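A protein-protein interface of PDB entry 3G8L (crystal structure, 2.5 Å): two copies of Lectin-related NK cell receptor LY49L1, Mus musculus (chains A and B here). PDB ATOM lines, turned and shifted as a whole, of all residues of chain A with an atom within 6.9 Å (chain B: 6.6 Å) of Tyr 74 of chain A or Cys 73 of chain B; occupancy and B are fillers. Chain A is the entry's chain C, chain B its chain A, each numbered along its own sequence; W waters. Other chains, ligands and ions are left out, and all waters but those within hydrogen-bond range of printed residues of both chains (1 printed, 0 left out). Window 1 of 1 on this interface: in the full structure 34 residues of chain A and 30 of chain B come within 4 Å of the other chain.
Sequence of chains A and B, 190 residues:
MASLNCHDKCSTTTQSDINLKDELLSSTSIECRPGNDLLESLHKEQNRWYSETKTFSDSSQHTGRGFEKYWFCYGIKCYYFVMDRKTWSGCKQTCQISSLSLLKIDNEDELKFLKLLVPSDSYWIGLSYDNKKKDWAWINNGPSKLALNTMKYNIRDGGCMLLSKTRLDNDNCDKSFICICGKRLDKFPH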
ATOM      1  N   TRP A  49     -22.788 -24.068  27.225  1.00  0.00           N
ATOM      2  CA  TRP A  49     -22.201 -25.214  26.532  1.00  0.00           C
ATOM      3  C   TRP A  49     -22.531 -26.509  27.316  1.00  0.00           C
ATOM      4  O   TRP A  49     -23.178 -27.435  26.756  1.00  0.00           O
ATOM      5  CB  TRP A  49     -20.720 -25.031  26.409  1.00  0.00           C
ATOM      6  CG  TRP A  49     -20.459 -23.739  25.704  1.00  0.00           C
ATOM      7  CD1 TRP A  49     -21.399 -22.989  24.904  1.00  0.00           C
ATOM      8  CD2 TRP A  49     -19.280 -23.031  25.662  1.00  0.00           C
ATOM      9  NE1 TRP A  49     -20.796 -21.858  24.456  1.00  0.00           N
ATOM     10  CE2 TRP A  49     -19.508 -21.865  24.881  1.00  0.00           C
ATOM     11  CE3 TRP A  49     -18.038 -23.209  26.249  1.00  0.00           C
ATOM     12  CZ2 TRP A  49     -18.561 -20.964  24.644  1.00  0.00           C
ATOM     13  CZ3 TRP A  49     -17.039 -22.284  25.972  1.00  0.00           C
ATOM     14  CH2 TRP A  49     -17.326 -21.161  25.203  1.00  0.00           C
ATOM     15  N   PHE A  72     -16.864 -28.760  24.397  1.00  0.00           N
ATOM     16  CA  PHE A  72     -16.977 -27.534  23.735  1.00  0.00           C
ATOM     17  C   PHE A  72     -15.681 -27.394  23.102  1.00  0.00           C
ATOM     18  O   PHE A  72     -14.806 -28.293  23.355  1.00  0.00           O
ATOM     19  CB  PHE A  72     -17.134 -26.428  24.698  1.00  0.00           C
ATOM     20  CG  PHE A  72     -15.974 -26.230  25.594  1.00  0.00           C
ATOM     21  CD1 PHE A  72     -14.882 -25.549  25.186  1.00  0.00           C
ATOM     22  CD2 PHE A  72     -16.003 -26.760  26.890  1.00  0.00           C
ATOM     23  CE1 PHE A  72     -13.795 -25.367  26.037  1.00  0.00           C
ATOM     24  CE2 PHE A  72     -15.053 -26.555  27.715  1.00  0.00           C
ATOM     25  CZ  PHE A  72     -13.925 -25.874  27.292  1.00  0.00           C
ATOM     26  N   CYS A  73     -15.552 -26.333  22.224  1.00  0.00           N
ATOM     27  CA  CYS A  73     -14.301 -26.093  21.427  1.00  0.00           C
ATOM     28  C   CYS A  73     -13.613 -24.821  21.580  1.00  0.00           C
ATOM     29  O   CYS A  73     -14.008 -23.889  22.313  1.00  0.00           O
ATOM     30  CB  CYS A  73     -14.436 -26.436  19.953  1.00  0.00           C
ATOM     31  SG  CYS A  73     -15.431 -27.914  19.368  1.00  0.00           S
ATOM     32  N   TYR A  74     -12.440 -24.728  21.016  1.00  0.00           N
ATOM     33  CA  TYR A  74     -11.781 -23.444  21.275  1.00  0.00           C
ATOM     34  C   TYR A  74     -10.587 -23.129  20.367  1.00  0.00           C
ATOM     35  O   TYR A  74      -9.390 -23.482  20.681  1.00  0.00           O
ATOM     36  CB  TYR A  74     -11.433 -23.408  22.727  1.00  0.00           C
ATOM     37  CG  TYR A  74     -10.686 -22.158  23.084  1.00  0.00           C
ATOM     38  CD1 TYR A  74      -9.224 -22.164  23.289  1.00  0.00           C
ATOM     39  CD2 TYR A  74     -11.375 -20.950  23.239  1.00  0.00           C
ATOM     40  CE1 TYR A  74      -8.482 -20.882  23.628  1.00  0.00           C
ATOM     41  CE2 TYR A  74     -10.668 -19.787  23.538  1.00  0.00           C
ATOM     42  CZ  TYR A  74      -9.235 -19.792  23.746  1.00  0.00           C
ATOM     43  OH  TYR A  74      -8.641 -18.624  24.052  1.00  0.00           O
ATOM     44  N   GLY A  75     -10.836 -22.431  19.254  1.00  0.00           N
ATOM     45  CA  GLY A  75      -9.690 -22.365  18.340  1.00  0.00           C
ATOM     46  C   GLY A  75      -9.901 -23.478  17.412  1.00  0.00           C
ATOM     47  O   GLY A  75     -10.969 -23.585  16.921  1.00  0.00           O
ATOM     48  N   ILE A  76      -8.897 -24.333  17.198  1.00  0.00           N
ATOM     49  CA  ILE A  76      -8.929 -25.547  16.484  1.00  0.00           C
ATOM     50  C   ILE A  76      -8.906 -26.927  17.344  1.00  0.00           C
ATOM     51  O   ILE A  76      -8.284 -27.952  16.959  1.00  0.00           O
ATOM     52  CB  ILE A  76      -7.680 -25.437  15.609  1.00  0.00           C
ATOM     53  CG1 ILE A  76      -6.355 -25.497  16.340  1.00  0.00           C
ATOM     54  CG2 ILE A  76      -7.574 -24.086  15.140  1.00  0.00           C
ATOM     55  CD1 ILE A  76      -4.982 -24.969  15.398  1.00  0.00           C
ATOM     56  N   LYS A  77      -9.598 -26.956  18.465  1.00  0.00           N
ATOM     57  CA  LYS A  77      -9.506 -27.978  19.468  1.00  0.00           C
ATOM     58  C   LYS A  77     -10.854 -28.160  20.164  1.00  0.00           C
ATOM     59  O   LYS A  77     -11.508 -27.216  20.421  1.00  0.00           O
ATOM     60  CB  LYS A  77      -8.490 -27.483  20.461  1.00  0.00           C
ATOM     61  CG  LYS A  77      -6.972 -27.827  20.036  1.00  0.00           C
ATOM     62  CD  LYS A  77      -5.895 -27.553  21.020  1.00  0.00           C
ATOM     63  CE  LYS A  77      -5.778 -28.835  21.978  1.00  0.00           C
ATOM     64  NZ  LYS A  77      -5.197 -28.522  23.397  1.00  0.00           N
ATOM     65  N   CYS A  78     -11.358 -29.367  20.383  1.00  0.00           N
ATOM     66  CA  CYS A  78     -12.506 -29.460  21.295  1.00  0.00           C
ATOM     67  C   CYS A  78     -12.003 -30.162  22.550  1.00  0.00           C
ATOM     68  O   CYS A  78     -10.856 -30.609  22.560  1.00  0.00           O
ATOM     69  CB  CYS A  78     -13.671 -30.187  20.657  1.00  0.00           C
ATOM     70  SG  CYS A  78     -14.097 -29.531  18.995  1.00  0.00           S
ATOM     71  N   TYR A  79     -12.876 -30.242  23.568  1.00  0.00           N
ATOM     72  CA  TYR A  79     -12.602 -30.658  24.897  1.00  0.00           C
ATOM     73  C   TYR A  79     -13.766 -31.470  25.231  1.00  0.00           C
ATOM     74  O   TYR A  79     -14.886 -30.966  25.183  1.00  0.00           O
ATOM     75  CB  TYR A  79     -12.617 -29.449  25.672  1.00  0.00           C
ATOM     76  CG  TYR A  79     -11.443 -28.577  25.263  1.00  0.00           C
ATOM     77  CD1 TYR A  79     -11.631 -27.457  24.450  1.00  0.00           C
ATOM     78  CD2 TYR A  79     -10.207 -28.834  25.695  1.00  0.00           C
ATOM     79  CE1 TYR A  79     -10.599 -26.620  24.103  1.00  0.00           C
ATOM     80  CE2 TYR A  79      -9.145 -27.984  25.397  1.00  0.00           C
ATOM     81  CZ  TYR A  79      -9.362 -26.871  24.576  1.00  0.00           C
ATOM     82  OH  TYR A  79      -8.318 -26.058  24.142  1.00  0.00           O
ATOM     83  N   ASP A 109      -1.722 -19.596  26.613  1.00  0.00           N
ATOM     84  CA  ASP A 109      -3.023 -18.997  26.418  1.00  0.00           C
ATOM     85  C   ASP A 109      -4.203 -19.943  26.523  1.00  0.00           C
ATOM     86  O   ASP A 109      -5.136 -19.727  27.305  1.00  0.00           O
ATOM     87  CB  ASP A 109      -3.021 -18.106  25.193  1.00  0.00           C
ATOM     88  CG  ASP A 109      -2.198 -16.815  25.430  1.00  0.00           C
ATOM     89  OD1 ASP A 109      -1.210 -16.621  24.623  1.00  0.00           O
ATOM     90  OD2 ASP A 109      -2.545 -16.018  26.419  1.00  0.00           O
ATOM     91  N   GLU A 110      -4.075 -21.077  25.895  1.00  0.00           N
ATOM     92  CA  GLU A 110      -5.142 -21.990  25.949  1.00  0.00           C
ATOM     93  C   GLU A 110      -5.369 -22.327  27.353  1.00  0.00           C
ATOM     94  O   GLU A 110      -6.542 -22.735  27.735  1.00  0.00           O
ATOM     95  CB  GLU A 110      -4.757 -23.198  25.188  1.00  0.00           C
ATOM     96  CG  GLU A 110      -5.569 -24.346  25.497  1.00  0.00           C
ATOM     97  CD  GLU A 110      -4.992 -25.543  24.848  1.00  0.00           C
ATOM     98  OE1 GLU A 110      -3.787 -25.697  24.471  1.00  0.00           O
ATOM     99  OE2 GLU A 110      -5.793 -26.383  24.620  1.00  0.00           O
ATOM    100  N   LEU A 111      -4.299 -22.177  28.162  1.00  0.00           N
ATOM    101  CA  LEU A 111      -4.379 -22.411  29.612  1.00  0.00           C
ATOM    102  C   LEU A 111      -4.988 -21.327  30.444  1.00  0.00           C
ATOM    103  O   LEU A 111      -5.788 -21.589  31.416  1.00  0.00           O
ATOM    104  CB  LEU A 111      -2.996 -22.748  30.120  1.00  0.00           C
ATOM    105  CG  LEU A 111      -2.769 -22.738  31.619  1.00  0.00           C
ATOM    106  CD1 LEU A 111      -2.681 -24.124  32.206  1.00  0.00           C
ATOM    107  CD2 LEU A 111      -1.376 -21.950  31.712  1.00  0.00           C
ATOM    108  N   PHE A 113      -7.323 -19.372  29.579  1.00  0.00           N
ATOM    109  CA  PHE A 113      -8.685 -19.552  29.287  1.00  0.00           C
ATOM    110  C   PHE A 113      -9.226 -20.748  29.969  1.00  0.00           C
ATOM    111  O   PHE A 113     -10.294 -20.715  30.514  1.00  0.00           O
ATOM    112  CB  PHE A 113      -8.758 -19.910  27.790  1.00  0.00           C
ATOM    113  CG  PHE A 113     -10.161 -20.118  27.288  1.00  0.00           C
ATOM    114  CD1 PHE A 113     -11.074 -19.054  27.151  1.00  0.00           C
ATOM    115  CD2 PHE A 113     -10.608 -21.348  26.983  1.00  0.00           C
ATOM    116  CE1 PHE A 113     -12.349 -19.246  26.742  1.00  0.00           C
ATOM    117  CE2 PHE A 113     -11.963 -21.513  26.506  1.00  0.00           C
ATOM    118  CZ  PHE A 113     -12.779 -20.482  26.394  1.00  0.00           C
ATOM    119  N   LEU A 114      -8.642 -21.912  29.779  1.00  0.00           N
ATOM    120  CA  LEU A 114      -9.320 -23.093  30.359  1.00  0.00           C
ATOM    121  C   LEU A 114      -9.303 -22.945  31.880  1.00  0.00           C
ATOM    122  O   LEU A 114     -10.321 -23.023  32.582  1.00  0.00           O
ATOM    123  CB  LEU A 114      -8.613 -24.350  30.005  1.00  0.00           C
ATOM    124  CG  LEU A 114      -8.464 -24.560  28.487  1.00  0.00           C
ATOM    125  CD1 LEU A 114      -7.407 -25.534  28.286  1.00  0.00           C
ATOM    126  CD2 LEU A 114      -9.709 -25.178  27.881  1.00  0.00           C
ATOM    127  N   LEU A 185      -8.307 -30.174  15.552  1.00  0.00           N
ATOM    128  CA  LEU A 185      -9.013 -30.651  14.340  1.00  0.00           C
ATOM    129  C   LEU A 185      -8.242 -30.160  13.207  1.00  0.00           C
ATOM    130  O   LEU A 185      -7.756 -29.027  13.223  1.00  0.00           O
ATOM    131  CB  LEU A 185     -10.396 -30.112  14.170  1.00  0.00           C
ATOM    132  CG  LEU A 185     -11.061 -29.730  15.433  1.00  0.00           C
ATOM    133  CD1 LEU A 185     -11.425 -28.192  15.335  1.00  0.00           C
ATOM    134  CD2 LEU A 185     -12.269 -30.404  15.351  1.00  0.00           C
ATOM    135  N   PHE A 188     -12.317 -28.081   8.799  1.00  0.00           N
ATOM    136  CA  PHE A 188     -13.415 -27.364   9.291  1.00  0.00           C
ATOM    137  C   PHE A 188     -14.409 -28.409   9.615  1.00  0.00           C
ATOM    138  O   PHE A 188     -14.669 -29.306   8.900  1.00  0.00           O
ATOM    139  CB  PHE A 188     -14.009 -26.376   8.248  1.00  0.00           C
ATOM    140  CG  PHE A 188     -15.124 -25.533   8.811  1.00  0.00           C
ATOM    141  CD1 PHE A 188     -16.419 -25.888   8.634  1.00  0.00           C
ATOM    142  CD2 PHE A 188     -14.863 -24.442   9.692  1.00  0.00           C
ATOM    143  CE1 PHE A 188     -17.416 -25.199   9.200  1.00  0.00           C
ATOM    144  CE2 PHE A 188     -15.863 -23.718  10.255  1.00  0.00           C
ATOM    145  CZ  PHE A 188     -17.187 -24.055   9.988  1.00  0.00           C
ATOM    146  N   PRO A 189     -14.996 -28.312  10.777  1.00  0.00           N
ATOM    147  CA  PRO A 189     -15.879 -29.434  11.078  1.00  0.00           C
ATOM    148  C   PRO A 189     -16.945 -29.785  10.075  1.00  0.00           C
ATOM    149  O   PRO A 189     -18.140 -29.541  10.338  1.00  0.00           O
ATOM    150  CB  PRO A 189     -16.454 -29.084  12.428  1.00  0.00           C
ATOM    151  CG  PRO A 189     -15.444 -28.041  13.001  1.00  0.00           C
ATOM    152  CD  PRO A 189     -14.771 -27.364  11.887  1.00  0.00           C
ATOM    153  N   LEU B  38      -7.741 -12.394  29.805  1.00  0.00           N
ATOM    154  CA  LEU B  38      -8.477 -13.025  28.772  1.00  0.00           C
ATOM    155  C   LEU B  38      -8.223 -12.326  27.491  1.00  0.00           C
ATOM    156  O   LEU B  38      -7.744 -12.950  26.563  1.00  0.00           O
ATOM    157  CB  LEU B  38      -9.928 -13.133  29.117  1.00  0.00           C
ATOM    158  CG  LEU B  38     -10.465 -14.485  28.648  1.00  0.00           C
ATOM    159  CD1 LEU B  38      -9.440 -15.521  28.164  1.00  0.00           C
ATOM    160  CD2 LEU B  38     -11.310 -14.991  29.746  1.00  0.00           C
ATOM    161  N   SER B  41      -5.010 -12.805  25.837  1.00  0.00           N
ATOM    162  CA  SER B  41      -5.012 -14.159  25.291  1.00  0.00           C
ATOM    163  C   SER B  41      -5.863 -14.315  24.100  1.00  0.00           C
ATOM    164  O   SER B  41      -5.323 -14.750  23.083  1.00  0.00           O
ATOM    165  CB  SER B  41      -5.536 -15.151  26.297  1.00  0.00           C
ATOM    166  OG  SER B  41      -4.696 -15.176  27.403  1.00  0.00           O
ATOM    167  N   LEU B  42      -7.182 -14.062  24.258  1.00  0.00           N
ATOM    168  CA  LEU B  42      -8.145 -13.877  23.157  1.00  0.00           C
ATOM    169  C   LEU B  42      -7.439 -13.347  21.938  1.00  0.00           C
ATOM    170  O   LEU B  42      -7.060 -14.086  21.021  1.00  0.00           O
ATOM    171  CB  LEU B  42      -9.298 -12.984  23.601  1.00  0.00           C
ATOM    172  CG  LEU B  42     -10.438 -13.777  24.322  1.00  0.00           C
ATOM    173  CD1 LEU B  42     -10.148 -15.275  24.772  1.00  0.00           C
ATOM    174  CD2 LEU B  42     -11.296 -12.999  25.408  1.00  0.00           C
ATOM    175  N   GLU B  45      -4.745 -15.757  20.772  1.00  0.00           N
ATOM    176  CA  GLU B  45      -5.036 -17.068  20.313  1.00  0.00           C
ATOM    177  C   GLU B  45      -5.638 -16.804  18.970  1.00  0.00           C
ATOM    178  O   GLU B  45      -5.666 -17.729  18.087  1.00  0.00           O
ATOM    179  CB  GLU B  45      -6.013 -17.741  21.236  1.00  0.00           C
ATOM    180  CG  GLU B  45      -5.329 -18.216  22.401  1.00  0.00           C
ATOM    181  CD  GLU B  45      -4.749 -19.598  22.185  1.00  0.00           C
ATOM    182  OE1 GLU B  45      -5.377 -20.636  22.640  1.00  0.00           O
ATOM    183  OE2 GLU B  45      -3.699 -19.656  21.491  1.00  0.00           O
ATOM    184  N   TRP B  49      -5.085 -18.590  15.457  1.00  0.00           N
ATOM    185  CA  TRP B  49      -5.879 -19.513  14.674  1.00  0.00           C
ATOM    186  C   TRP B  49      -6.041 -19.073  13.227  1.00  0.00           C
ATOM    187  O   TRP B  49      -6.275 -19.939  12.311  1.00  0.00           O
ATOM    188  CB  TRP B  49      -7.261 -19.593  15.249  1.00  0.00           C
ATOM    189  CG  TRP B  49      -7.287 -19.846  16.667  1.00  0.00           C
ATOM    190  CD1 TRP B  49      -6.370 -20.630  17.459  1.00  0.00           C
ATOM    191  CD2 TRP B  49      -8.282 -19.407  17.538  1.00  0.00           C
ATOM    192  NE1 TRP B  49      -6.813 -20.709  18.724  1.00  0.00           N
ATOM    193  CE2 TRP B  49      -7.978 -19.959  18.830  1.00  0.00           C
ATOM    194  CE3 TRP B  49      -9.418 -18.635  17.372  1.00  0.00           C
ATOM    195  CZ2 TRP B  49      -8.798 -19.688  19.976  1.00  0.00           C
ATOM    196  CZ3 TRP B  49     -10.281 -18.396  18.499  1.00  0.00           C
ATOM    197  CH2 TRP B  49      -9.951 -18.925  19.775  1.00  0.00           C
ATOM    198  N   TRP B  71     -11.096 -19.625   9.809  1.00  0.00           N
ATOM    199  CA  TRP B  71     -12.165 -20.169  10.655  1.00  0.00           C
ATOM    200  C   TRP B  71     -11.669 -20.469  12.081  1.00  0.00           C
ATOM    201  O   TRP B  71     -10.376 -20.394  12.402  1.00  0.00           O
ATOM    202  CB  TRP B  71     -12.823 -21.402  10.012  1.00  0.00           C
ATOM    203  CG  TRP B  71     -11.882 -22.592   9.910  1.00  0.00           C
ATOM    204  CD1 TRP B  71     -11.031 -22.950   8.814  1.00  0.00           C
ATOM    205  CD2 TRP B  71     -11.664 -23.649  10.921  1.00  0.00           C
ATOM    206  NE1 TRP B  71     -10.306 -24.113   9.134  1.00  0.00           N
ATOM    207  CE2 TRP B  71     -10.651 -24.548  10.407  1.00  0.00           C
ATOM    208  CE3 TRP B  71     -12.212 -23.920  12.173  1.00  0.00           C
ATOM    209  CZ2 TRP B  71     -10.166 -25.690  11.175  1.00  0.00           C
ATOM    210  CZ3 TRP B  71     -11.698 -25.120  12.959  1.00  0.00           C
ATOM    211  CH2 TRP B  71     -10.689 -25.923  12.453  1.00  0.00           C
ATOM    212  N   PHE B  72     -12.616 -20.728  12.982  1.00  0.00           N
ATOM    213  CA  PHE B  72     -12.184 -21.160  14.253  1.00  0.00           C
ATOM    214  C   PHE B  72     -13.483 -21.318  14.953  1.00  0.00           C
ATOM    215  O   PHE B  72     -14.410 -20.840  14.357  1.00  0.00           O
ATOM    216  CB  PHE B  72     -11.340 -20.075  14.870  1.00  0.00           C
ATOM    217  CG  PHE B  72     -12.122 -18.803  15.217  1.00  0.00           C
ATOM    218  CD1 PHE B  72     -13.080 -18.808  16.180  1.00  0.00           C
ATOM    219  CD2 PHE B  72     -11.857 -17.622  14.579  1.00  0.00           C
ATOM    220  CE1 PHE B  72     -13.683 -17.674  16.540  1.00  0.00           C
ATOM    221  CE2 PHE B  72     -12.536 -16.549  14.844  1.00  0.00           C
ATOM    222  CZ  PHE B  72     -13.440 -16.577  15.872  1.00  0.00           C
ATOM    223  N   CYS B  73     -13.520 -22.025  16.101  1.00  0.00           N
ATOM    224  CA  CYS B  73     -14.718 -22.378  16.794  1.00  0.00           C
ATOM    225  C   CYS B  73     -14.704 -21.879  18.170  1.00  0.00           C
ATOM    226  O   CYS B  73     -13.638 -21.626  18.736  1.00  0.00           O
ATOM    227  CB  CYS B  73     -14.908 -23.901  16.912  1.00  0.00           C
ATOM    228  SG  CYS B  73     -14.817 -24.825  15.388  1.00  0.00           S
ATOM    229  N   TYR B  74     -15.889 -21.772  18.753  1.00  0.00           N
ATOM    230  CA  TYR B  74     -15.948 -21.187  20.055  1.00  0.00           C
ATOM    231  C   TYR B  74     -17.243 -21.601  20.647  1.00  0.00           C
ATOM    232  O   TYR B  74     -18.364 -21.209  20.142  1.00  0.00           O
ATOM    233  CB  TYR B  74     -15.900 -19.739  19.923  1.00  0.00           C
ATOM    234  CG  TYR B  74     -15.822 -19.125  21.225  1.00  0.00           C
ATOM    235  CD1 TYR B  74     -16.939 -18.703  21.900  1.00  0.00           C
ATOM    236  CD2 TYR B  74     -14.538 -18.870  21.772  1.00  0.00           C
ATOM    237  CE1 TYR B  74     -16.793 -18.142  23.203  1.00  0.00           C
ATOM    238  CE2 TYR B  74     -14.368 -18.313  22.993  1.00  0.00           C
ATOM    239  CZ  TYR B  74     -15.462 -17.970  23.730  1.00  0.00           C
ATOM    240  OH  TYR B  74     -15.111 -17.356  24.999  1.00  0.00           O
ATOM    241  N   GLY B  75     -17.137 -22.589  21.554  1.00  0.00           N
ATOM    242  CA  GLY B  75     -18.316 -23.099  22.134  1.00  0.00           C
ATOM    243  C   GLY B  75     -18.852 -24.212  21.272  1.00  0.00           C
ATOM    244  O   GLY B  75     -18.175 -25.108  21.076  1.00  0.00           O
ATOM    245  N   ILE B  76     -20.129 -24.229  20.929  1.00  0.00           N
ATOM    246  CA  ILE B  76     -20.743 -25.223  20.002  1.00  0.00           C
ATOM    247  C   ILE B  76     -20.752 -24.622  18.560  1.00  0.00           C
ATOM    248  O   ILE B  76     -21.286 -25.245  17.615  1.00  0.00           O
ATOM    249  CB  ILE B  76     -22.225 -25.491  20.367  1.00  0.00           C
ATOM    250  CG1 ILE B  76     -23.043 -24.129  20.764  1.00  0.00           C
ATOM    251  CG2 ILE B  76     -22.341 -26.465  21.586  1.00  0.00           C
ATOM    252  CD1 ILE B  76     -22.095 -22.574  21.306  1.00  0.00           C
ATOM    253  N   LYS B  77     -20.151 -23.470  18.334  1.00  0.00           N
ATOM    254  CA  LYS B  77     -20.325 -22.863  17.004  1.00  0.00           C
ATOM    255  C   LYS B  77     -18.944 -22.798  16.407  1.00  0.00           C
ATOM    256  O   LYS B  77     -17.960 -22.491  17.202  1.00  0.00           O
ATOM    257  CB  LYS B  77     -20.939 -21.409  17.105  1.00  0.00           C
ATOM    258  CG  LYS B  77     -22.519 -21.404  17.441  1.00  0.00           C
ATOM    259  CD  LYS B  77     -23.509 -21.131  16.069  1.00  0.00           C
ATOM    260  CE  LYS B  77     -23.862 -19.706  15.852  1.00  0.00           C
ATOM    261  NZ  LYS B  77     -23.691 -18.469  17.029  1.00  0.00           N
ATOM    262  N   CYS B  78     -18.842 -23.025  15.081  1.00  0.00           N
ATOM    263  CA  CYS B  78     -17.664 -22.615  14.376  1.00  0.00           C
ATOM    264  C   CYS B  78     -18.031 -21.464  13.394  1.00  0.00           C
ATOM    265  O   CYS B  78     -19.152 -21.409  12.977  1.00  0.00           O
ATOM    266  CB  CYS B  78     -17.116 -23.783  13.616  1.00  0.00           C
ATOM    267  SG  CYS B  78     -16.815 -25.259  14.613  1.00  0.00           S
ATOM    268  N   TYR B  79     -17.069 -20.645  12.986  1.00  0.00           N
ATOM    269  CA  TYR B  79     -17.194 -19.422  12.262  1.00  0.00           C
ATOM    270  C   TYR B  79     -16.207 -19.532  11.186  1.00  0.00           C
ATOM    271  O   TYR B  79     -15.091 -19.754  11.485  1.00  0.00           O
ATOM    272  CB  TYR B  79     -16.655 -18.248  13.098  1.00  0.00           C
ATOM    273  CG  TYR B  79     -17.454 -18.219  14.331  1.00  0.00           C
ATOM    274  CD1 TYR B  79     -16.984 -18.807  15.513  1.00  0.00           C
ATOM    275  CD2 TYR B  79     -18.779 -17.713  14.316  1.00  0.00           C
ATOM    276  CE1 TYR B  79     -17.770 -18.852  16.678  1.00  0.00           C
ATOM    277  CE2 TYR B  79     -19.571 -17.772  15.463  1.00  0.00           C
ATOM    278  CZ  TYR B  79     -19.040 -18.381  16.639  1.00  0.00           C
ATOM    279  OH  TYR B  79     -19.775 -18.438  17.743  1.00  0.00           O
ATOM    280  N   LEU B 117     -12.933 -11.443  19.822  1.00  0.00           N
ATOM    281  CA  LEU B 117     -11.902 -12.095  18.991  1.00  0.00           C
ATOM    282  C   LEU B 117     -11.815 -11.792  17.486  1.00  0.00           C
ATOM    283  O   LEU B 117     -11.083 -12.448  16.714  1.00  0.00           O
ATOM    284  CB  LEU B 117     -11.851 -13.601  19.198  1.00  0.00           C
ATOM    285  CG  LEU B 117     -13.012 -14.540  19.365  1.00  0.00           C
ATOM    286  CD1 LEU B 117     -12.711 -15.289  20.631  1.00  0.00           C
ATOM    287  CD2 LEU B 117     -14.374 -13.831  19.540  1.00  0.00           C
ATOM    288  N   LEU B 185     -22.260 -26.916  15.658  1.00  0.00           N
ATOM    289  CA  LEU B 185     -21.836 -28.323  15.796  1.00  0.00           C
ATOM    290  C   LEU B 185     -23.066 -29.092  16.255  1.00  0.00           C
ATOM    291  O   LEU B 185     -23.844 -28.582  17.056  1.00  0.00           O
ATOM    292  CB  LEU B 185     -20.696 -28.417  16.795  1.00  0.00           C
ATOM    293  CG  LEU B 185     -19.546 -27.662  16.091  1.00  0.00           C
ATOM    294  CD1 LEU B 185     -18.101 -27.777  16.722  1.00  0.00           C
ATOM    295  CD2 LEU B 185     -19.612 -28.247  14.669  1.00  0.00           C
HETATM  296  O   HOH W   1      -6.315 -23.255  20.033  1.00  0.00           O
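The side-chain hydroxyl (OG) of Ser 41 of chain B is in hydrogen-bond range of the side-chain carboxylate (OD2) of Asp 109 of chain A. The backbone carbonyl oxygen (O) of Cys 73 of chain B sits at hydrogen-bond distance from the backbone NH (N) of Gly 75 of chain A (3.0 Å). O of Gly 75 of chain B sits at hydrogen-bond distance from N of Cys 73 of chain A.
The backbone carbonyl oxygen (O) of Phe 72 of chain B is in hydrogen-bond range of the backbone NH (N) of Tyr 79 of chain B, 3.0 Å away. The backbone carbonyl oxygen (O) of Phe 72 of chain A is in hydrogen-bond range of the backbone NH (N) of Tyr 79 of chain A (2.8 Å). The side-chain amino group of Lys 77 of chain A is in salt-bridge range of the side-chain carboxylate of Glu 110 of chain A, at 2.5 Å. OH of Tyr 79 of chain A lies within hydrogen-bond range of OE2 of Glu 110 of chain A (2.6 Å).
CA of Phe 72 of chain A touches O of Gly 75 of chain B (3.8 Å). OH of Tyr 74 of chain A touches CD1 of Leu 42 of chain B, 3.7 Å away. CE1 of Tyr 74 of chain A touches OE1 of Glu 45 of chain B (3.3 Å). Tyr 74 of chain A touches Trp 49 of chain B (CZ to CZ2, 3.8 Å). Glu 45 of chain B touches Asp 109 of chain A. Tyr 74 of chain B touches Phe 113 of chain A. CD2 of Phe 188 of chain A touches CG of Trp 71 of chain B, at 3.5 Å. CB of Cys 78 of chain B touches CE2 of Phe 188 of chain A, at 3.6 Å.
Of the printed residues of chain B, Trp 49 of chain A touches Tyr 74, Gly 75 and Ile 76. Cys 78 of chain A touches none of the printed residues of chain B. Printed residues of chain A within 4 Å of Ser 41 of chain B: Asp 109. Of the printed residues of chain A, Trp 49 of chain B touches Tyr 74 and Gly 75. Of the printed residues of chain A, Cys 73 of chain B touches Cys 73 (3.99 Å), Tyr 74 (3.6 Å) and Gly 75 (3.0 Å). The nearest printed residue of chain A that does not touch Cys 73 of chain B is Pro 189 of chain A (4.1 Å). The nearest printed residue of chain A that does not touch Trp 49 of chain B is Ile 76 of chain A (4.3 Å).
Of the 17 printed residues of chain A, 11 touch a printed residue of chain B. Printed residues of chain A that touch a printed residue of chain B: Trp 49, Phe 72, Cys 73, Tyr 74, Gly 75, Asp 109, Glu 110, Phe 113, Leu 185, Phe 188 and Pro 189. Hydrophobic or aromatic side chains of chain A that line the printed part of chain B: Trp 49, Phe 72, Tyr 74, Phe 113, Leu 185, Phe 188 and Pro 189. Along chain A the printed residues that touch a printed residue of chain B span positions 49 to 189. Printed residues of chain B that touch a printed residue of chain A: Ser 41, Leu 42, Glu 45, Trp 49, Trp 71, Phe 72, Cys 73, Tyr 74, Gly 75, Ile 76, Cys 78 and Leu 185. Among the printed residues, 25 pairs touch across the chains. Among the printed residues, no Asp or Glu carboxylate lies within 4 Å of a Lys or Arg side-chain nitrogen of the other chain.
Trp 49 of chain A touches Tyr 74 of chain B, and with the chains exchanged Tyr 74 of chain A touches Trp 49 of chain B. Trp 49 of chain A touches Gly 75 of chain B, and with the chains exchanged Gly 75 of chain A touches Trp 49 of chain B. Phe 72 of chain A touches Gly 75 of chain B, and with the chains exchanged Gly 75 of chain A touches Phe 72 of chain B. Of the 25 pairs that touch across the chains among the printed residues, 10 have their exchanged pair printed and touching as well.
Water W1 lies within hydrogen-bond range of the indole nitrogen (NE1) of Trp 49 of chain B (2.9 Å) and the backbone carbonyl oxygen (O) of Tyr 74 of chain A (3.2 Å).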
